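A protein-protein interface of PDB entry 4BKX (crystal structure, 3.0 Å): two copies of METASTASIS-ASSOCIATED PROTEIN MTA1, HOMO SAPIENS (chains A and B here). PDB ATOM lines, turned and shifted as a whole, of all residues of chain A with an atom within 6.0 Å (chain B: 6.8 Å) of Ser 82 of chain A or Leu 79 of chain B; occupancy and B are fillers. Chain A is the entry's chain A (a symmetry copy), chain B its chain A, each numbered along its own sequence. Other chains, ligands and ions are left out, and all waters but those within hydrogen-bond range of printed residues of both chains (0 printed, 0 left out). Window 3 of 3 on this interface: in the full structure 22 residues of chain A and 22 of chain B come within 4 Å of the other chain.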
ATOM      1  N   GLY A  62      35.707 -25.243 -30.223  1.00  0.00           N
ATOM      2  CA  GLY A  62      34.644 -24.258 -30.359  1.00  0.00           C
ATOM      3  C   GLY A  62      33.595 -24.349 -29.271  1.00  0.00           C
ATOM      4  O   GLY A  62      33.242 -23.333 -28.673  1.00  0.00           O
ATOM      5  N   THR A  63      33.096 -25.562 -29.013  1.00  0.00           N
ATOM      6  CA  THR A  63      32.047 -25.761 -28.001  1.00  0.00           C
ATOM      7  C   THR A  63      32.595 -25.488 -26.604  1.00  0.00           C
ATOM      8  O   THR A  63      31.927 -24.863 -25.780  1.00  0.00           O
ATOM      9  CB  THR A  63      31.407 -27.174 -28.028  1.00  0.00           C
ATOM     10  OG1 THR A  63      32.190 -28.079 -27.246  1.00  0.00           O
ATOM     11  CG2 THR A  63      31.287 -27.712 -29.431  1.00  0.00           C
ATOM     12  N   ARG A  66      32.909 -21.639 -25.989  1.00  0.00           N
ATOM     13  CA  ARG A  66      31.652 -21.001 -25.622  1.00  0.00           C
ATOM     14  C   ARG A  66      31.014 -21.625 -24.381  1.00  0.00           C
ATOM     15  O   ARG A  66      29.946 -21.196 -23.950  1.00  0.00           O
ATOM     16  CB  ARG A  66      30.677 -20.911 -26.809  1.00  0.00           C
ATOM     17  CG  ARG A  66      30.326 -22.215 -27.500  1.00  0.00           C
ATOM     18  CD  ARG A  66      29.896 -21.941 -28.934  1.00  0.00           C
ATOM     19  NE  ARG A  66      31.038 -21.923 -29.847  1.00  0.00           N
ATOM     20  CZ  ARG A  66      31.057 -21.324 -31.037  1.00  0.00           C
ATOM     21  NH1 ARG A  66      29.996 -20.660 -31.475  1.00  0.00           N
ATOM     22  NH2 ARG A  66      32.151 -21.379 -31.786  1.00  0.00           N
ATOM     23  N   ALA A  67      31.679 -22.631 -23.812  1.00  0.00           N
ATOM     24  CA  ALA A  67      31.338 -23.124 -22.481  1.00  0.00           C
ATOM     25  C   ALA A  67      31.988 -22.228 -21.432  1.00  0.00           C
ATOM     26  O   ALA A  67      31.453 -22.055 -20.341  1.00  0.00           O
ATOM     27  CB  ALA A  67      31.782 -24.566 -22.302  1.00  0.00           C
ATOM     28  N   SER A  78      21.212 -26.167 -24.047  1.00  0.00           N
ATOM     29  CA  SER A  78      22.255 -25.309 -24.598  1.00  0.00           C
ATOM     30  C   SER A  78      23.513 -26.093 -24.982  1.00  0.00           C
ATOM     31  O   SER A  78      24.381 -25.568 -25.686  1.00  0.00           O
ATOM     32  CB  SER A  78      22.594 -24.146 -23.644  1.00  0.00           C
ATOM     33  OG  SER A  78      23.332 -24.573 -22.508  1.00  0.00           O
ATOM     34  N   LEU A  79      23.611 -27.341 -24.526  1.00  0.00           N
ATOM     35  CA  LEU A  79      24.746 -28.188 -24.881  1.00  0.00           C
ATOM     36  C   LEU A  79      24.706 -28.545 -26.364  1.00  0.00           C
ATOM     37  O   LEU A  79      25.713 -28.403 -27.060  1.00  0.00           O
ATOM     38  CB  LEU A  79      24.810 -29.450 -24.014  1.00  0.00           C
ATOM     39  CG  LEU A  79      25.922 -30.461 -24.339  1.00  0.00           C
ATOM     40  CD1 LEU A  79      27.315 -29.861 -24.205  1.00  0.00           C
ATOM     41  CD2 LEU A  79      25.787 -31.692 -23.461  1.00  0.00           C
ATOM     42  N   HIS A  80      23.547 -28.999 -26.841  1.00  0.00           N
ATOM     43  CA  HIS A  80      23.353 -29.243 -28.269  1.00  0.00           C
ATOM     44  C   HIS A  80      23.424 -27.923 -29.043  1.00  0.00           C
ATOM     45  O   HIS A  80      23.976 -27.872 -30.142  1.00  0.00           O
ATOM     46  CB  HIS A  80      22.027 -29.963 -28.534  1.00  0.00           C
ATOM     47  N   MET A  81      22.884 -26.862 -28.440  1.00  0.00           N
ATOM     48  CA  MET A  81      22.875 -25.514 -29.019  1.00  0.00           C
ATOM     49  C   MET A  81      24.277 -24.969 -29.302  1.00  0.00           C
ATOM     50  O   MET A  81      24.533 -24.429 -30.382  1.00  0.00           O
ATOM     51  CB  MET A  81      22.147 -24.550 -28.084  1.00  0.00           C
ATOM     52  CG  MET A  81      20.652 -24.788 -27.939  1.00  0.00           C
ATOM     53  SD  MET A  81      19.650 -23.545 -28.781  1.00  0.00           S
ATOM     54  CE  MET A  81      20.152 -22.027 -27.959  1.00  0.00           C
ATOM     55  N   SER A  82      25.172 -25.102 -28.325  1.00  0.00           N
ATOM     56  CA  SER A  82      26.544 -24.609 -28.452  1.00  0.00           C
ATOM     57  C   SER A  82      27.392 -25.477 -29.373  1.00  0.00           C
ATOM     58  O   SER A  82      28.255 -24.968 -30.093  1.00  0.00           O
ATOM     59  CB  SER A  82      27.205 -24.486 -27.081  1.00  0.00           C
ATOM     60  OG  SER A  82      26.639 -23.418 -26.344  1.00  0.00           O
ATOM     61  N   ALA A  83      27.142 -26.786 -29.340  1.00  0.00           N
ATOM     62  CA  ALA A  83      27.810 -27.726 -30.241  1.00  0.00           C
ATOM     63  C   ALA A  83      27.432 -27.447 -31.693  1.00  0.00           C
ATOM     64  O   ALA A  83      28.302 -27.378 -32.557  1.00  0.00           O
ATOM     65  CB  ALA A  83      27.489 -29.165 -29.861  1.00  0.00           C
ATOM     66  N   ALA A  84      26.135 -27.269 -31.946  1.00  0.00           N
ATOM     67  CA  ALA A  84      25.646 -26.900 -33.270  1.00  0.00           C
ATOM     68  C   ALA A  84      26.221 -25.558 -33.702  1.00  0.00           C
ATOM     69  O   ALA A  84      26.599 -25.388 -34.865  1.00  0.00           O
ATOM     70  CB  ALA A  84      24.128 -26.860 -33.291  1.00  0.00           C
ATOM     71  N   ALA A  85      26.294 -24.615 -32.760  1.00  0.00           N
ATOM     72  CA  ALA A  85      26.895 -23.305 -33.005  1.00  0.00           C
ATOM     73  C   ALA A  85      28.344 -23.443 -33.458  1.00  0.00           C
ATOM     74  O   ALA A  85      28.744 -22.851 -34.459  1.00  0.00           O
ATOM     75  CB  ALA A  85      26.807 -22.432 -31.763  1.00  0.00           C
ATOM     76  N   ALA A  86      29.120 -24.241 -32.728  1.00  0.00           N
ATOM     77  CA  ALA A  86      30.520 -24.482 -33.073  1.00  0.00           C
ATOM     78  C   ALA A  86      30.687 -25.323 -34.343  1.00  0.00           C
ATOM     79  O   ALA A  86      31.771 -25.367 -34.924  1.00  0.00           O
ATOM     80  CB  ALA A  86      31.245 -25.126 -31.905  1.00  0.00           C
ATOM     81  N   SER A  87      29.613 -25.983 -34.769  1.00  0.00           N
ATOM     82  CA  SER A  87      29.632 -26.812 -35.976  1.00  0.00           C
ATOM     83  C   SER A  87      29.405 -26.015 -37.261  1.00  0.00           C
ATOM     84  O   SER A  87      29.640 -26.528 -38.359  1.00  0.00           O
ATOM     85  CB  SER A  87      28.595 -27.933 -35.873  1.00  0.00           C
ATOM     86  OG  SER A  87      28.945 -28.861 -34.865  1.00  0.00           O
ATOM     87  N   GLU A 127      24.805 -15.848 -34.833  1.00  0.00           N
ATOM     88  CA  GLU A 127      25.052 -16.142 -33.424  1.00  0.00           C
ATOM     89  C   GLU A 127      25.451 -14.888 -32.655  1.00  0.00           C
ATOM     90  O   GLU A 127      25.162 -14.767 -31.465  1.00  0.00           O
ATOM     91  CB  GLU A 127      26.147 -17.208 -33.289  1.00  0.00           C
ATOM     92  CG  GLU A 127      26.342 -17.738 -31.872  1.00  0.00           C
ATOM     93  CD  GLU A 127      27.526 -18.686 -31.728  1.00  0.00           C
ATOM     94  OE1 GLU A 127      28.282 -18.871 -32.709  1.00  0.00           O
ATOM     95  OE2 GLU A 127      27.701 -19.251 -30.624  1.00  0.00           O
ATOM     96  N   THR B  63      33.942 -32.615 -23.916  1.00  0.00           N
ATOM     97  CA  THR B  63      32.646 -31.923 -23.857  1.00  0.00           C
ATOM     98  C   THR B  63      31.860 -32.146 -25.146  1.00  0.00           C
ATOM     99  O   THR B  63      30.652 -32.376 -25.112  1.00  0.00           O
ATOM    100  CB  THR B  63      32.758 -30.399 -23.589  1.00  0.00           C
ATOM    101  OG1 THR B  63      32.958 -29.701 -24.820  1.00  0.00           O
ATOM    102  CG2 THR B  63      33.891 -30.074 -22.648  1.00  0.00           C
ATOM    103  N   SER B  78      23.442 -27.302 -18.648  1.00  0.00           N
ATOM    104  CA  SER B  78      24.177 -28.534 -18.910  1.00  0.00           C
ATOM    105  C   SER B  78      25.470 -28.287 -19.692  1.00  0.00           C
ATOM    106  O   SER B  78      26.324 -29.174 -19.775  1.00  0.00           O
ATOM    107  CB  SER B  78      23.292 -29.583 -19.614  1.00  0.00           C
ATOM    108  OG  SER B  78      23.046 -29.259 -20.975  1.00  0.00           O
ATOM    109  N   LEU B  79      25.614 -27.090 -20.260  1.00  0.00           N
ATOM    110  CA  LEU B  79      26.834 -26.737 -20.981  1.00  0.00           C
ATOM    111  C   LEU B  79      28.012 -26.620 -20.018  1.00  0.00           C
ATOM    112  O   LEU B  79      29.073 -27.197 -20.267  1.00  0.00           O
ATOM    113  CB  LEU B  79      26.663 -25.453 -21.800  1.00  0.00           C
ATOM    114  CG  LEU B  79      27.902 -24.937 -22.549  1.00  0.00           C
ATOM    115  CD1 LEU B  79      28.434 -25.942 -23.563  1.00  0.00           C
ATOM    116  CD2 LEU B  79      27.595 -23.613 -23.225  1.00  0.00           C
ATOM    117  N   HIS B  80      27.822 -25.882 -18.924  1.00  0.00           N
ATOM    118  CA  HIS B  80      28.831 -25.810 -17.869  1.00  0.00           C
ATOM    119  C   HIS B  80      28.994 -27.179 -17.202  1.00  0.00           C
ATOM    120  O   HIS B  80      30.109 -27.581 -16.865  1.00  0.00           O
ATOM    121  CB  HIS B  80      28.475 -24.736 -16.836  1.00  0.00           C
ATOM    122  N   MET B  81      27.876 -27.891 -17.047  1.00  0.00           N
ATOM    123  CA  MET B  81      27.841 -29.230 -16.448  1.00  0.00           C
ATOM    124  C   MET B  81      28.700 -30.251 -17.199  1.00  0.00           C
ATOM    125  O   MET B  81      29.459 -31.005 -16.582  1.00  0.00           O
ATOM    126  CB  MET B  81      26.402 -29.738 -16.392  1.00  0.00           C
ATOM    127  CG  MET B  81      25.486 -28.993 -15.434  1.00  0.00           C
ATOM    128  SD  MET B  81      25.084 -29.941 -13.951  1.00  0.00           S
ATOM    129  CE  MET B  81      24.275 -31.394 -14.633  1.00  0.00           C
ATOM    130  N   SER B  82      28.565 -30.278 -18.524  1.00  0.00           N
ATOM    131  CA  SER B  82      29.310 -31.216 -19.364  1.00  0.00           C
ATOM    132  C   SER B  82      30.778 -30.835 -19.503  1.00  0.00           C
ATOM    133  O   SER B  82      31.647 -31.709 -19.574  1.00  0.00           O
ATOM    134  CB  SER B  82      28.662 -31.342 -20.741  1.00  0.00           C
ATOM    135  OG  SER B  82      27.428 -32.031 -20.655  1.00  0.00           O
ATOM    136  N   ALA B  83      31.045 -29.530 -19.543  1.00  0.00           N
ATOM    137  CA  ALA B  83      32.415 -29.018 -19.574  1.00  0.00           C
ATOM    138  C   ALA B  83      33.156 -29.374 -18.287  1.00  0.00           C
ATOM    139  O   ALA B  83      34.282 -29.863 -18.336  1.00  0.00           O
ATOM    140  CB  ALA B  83      32.430 -27.515 -19.814  1.00  0.00           C
ATOM    141  N   ALA B  84      32.509 -29.143 -17.146  1.00  0.00           N
ATOM    142  CA  ALA B  84      33.059 -29.525 -15.849  1.00  0.00           C
ATOM    143  C   ALA B  84      33.266 -31.032 -15.776  1.00  0.00           C
ATOM    144  O   ALA B  84      34.282 -31.494 -15.250  1.00  0.00           O
ATOM    145  CB  ALA B  84      32.156 -29.056 -14.722  1.00  0.00           C
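Printed residues of chain A that touch a printed residue of chain B: Thr 63, Arg 66, Ala 67, Ser 78, Leu 79 and Ser 82.
Hydrophobic or aromatic side chains of chain A that line the printed part of chain B: Ala 67 and Leu 79.
Printed residues of chain B that touch a printed residue of chain A: Thr 63, Ser 78, Leu 79, Ser 82 and Ala 83.
Among the printed residues, 8 pairs touch across the chains.
Among the printed residues, no Asp or Glu carboxylate lies within 4 Å of a Lys or Arg side-chain nitrogen of the other chain.
The side-chain hydroxyl of Thr 63 of chain B sits at hydrogen-bond distance from the side-chain hydroxyl of Thr 63 of chain A (3.0 Å).
OG of Ser 82 of chain B sits at hydrogen-bond distance from O of Ser 78 of chain B, at 3.2 Å.
The backbone carbonyl oxygen (O) of Gly 62 of chain A lies within hydrogen-bond range of the guanidinium group (NE) of Arg 66 of chain A, 2.9 Å away.
The guanidinium group of Arg 66 of chain A lies within salt-bridge range of the side-chain carboxylate of Glu 127 of chain A, at 2.8 Å.
The backbone carbonyl oxygen of Ser 78 of chain A sits at hydrogen-bond distance from the side-chain hydroxyl of Ser 82 of chain A (3.2 Å).
Among the printed residues, merely in contact across the chains: Arg 66 of chain A with Leu 79 of chain B (3.4 Å), Ala 67 of chain A with Leu 79 of chain B (3.8 Å), Ala 67 of chain A with Ala 83 of chain B (3.9 Å), Ser 78 of chain A with Leu 79 of chain B (3.5 Å), Leu 79 of chain A with Ser 78 of chain B (3.5 Å), Leu 79 of chain A with Ser 82 of chain B (3.3 Å) and Ser 82 of chain A with Leu 79 of chain B (3.3 Å).
Thr 63 of chain B touches its own counterpart, Thr 63 of chain A.
Ser 78 of chain A touches Leu 79 of chain B, and with the chains exchanged Leu 79 of chain A touches Ser 78 of chain B.
Leu 79 of chain A touches Ser 82 of chain B, and with the chains exchanged Ser 82 of chain A touches Leu 79 of chain B.
Positions printed for both chains: 63, 78, 79, 80, 81, 82, 83 and 84.
Of the 8 pairs that touch across the chains among the printed residues, 5 have their exchanged pair printed and touching as well.
Ser 82 of chain A touches one residue of chain B.
Leu 79 of chain B touches four residues of chain A.
Of the printed residues of chain B, Ser 78 of chain A touches Leu 79.
Of the printed residues of chain A, Ala 83 of chain B touches Ala 67.
Ser 87 of chain A touches none of the printed residues of chain B.
The nearest residue of chain A that does not touch Leu 79 of chain B is Leu 79 of chain A (4.1 Å).
The nearest printed residue of chain A that does not touch Ser 82 of chain B is Ala 67 of chain A (6.9 Å).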
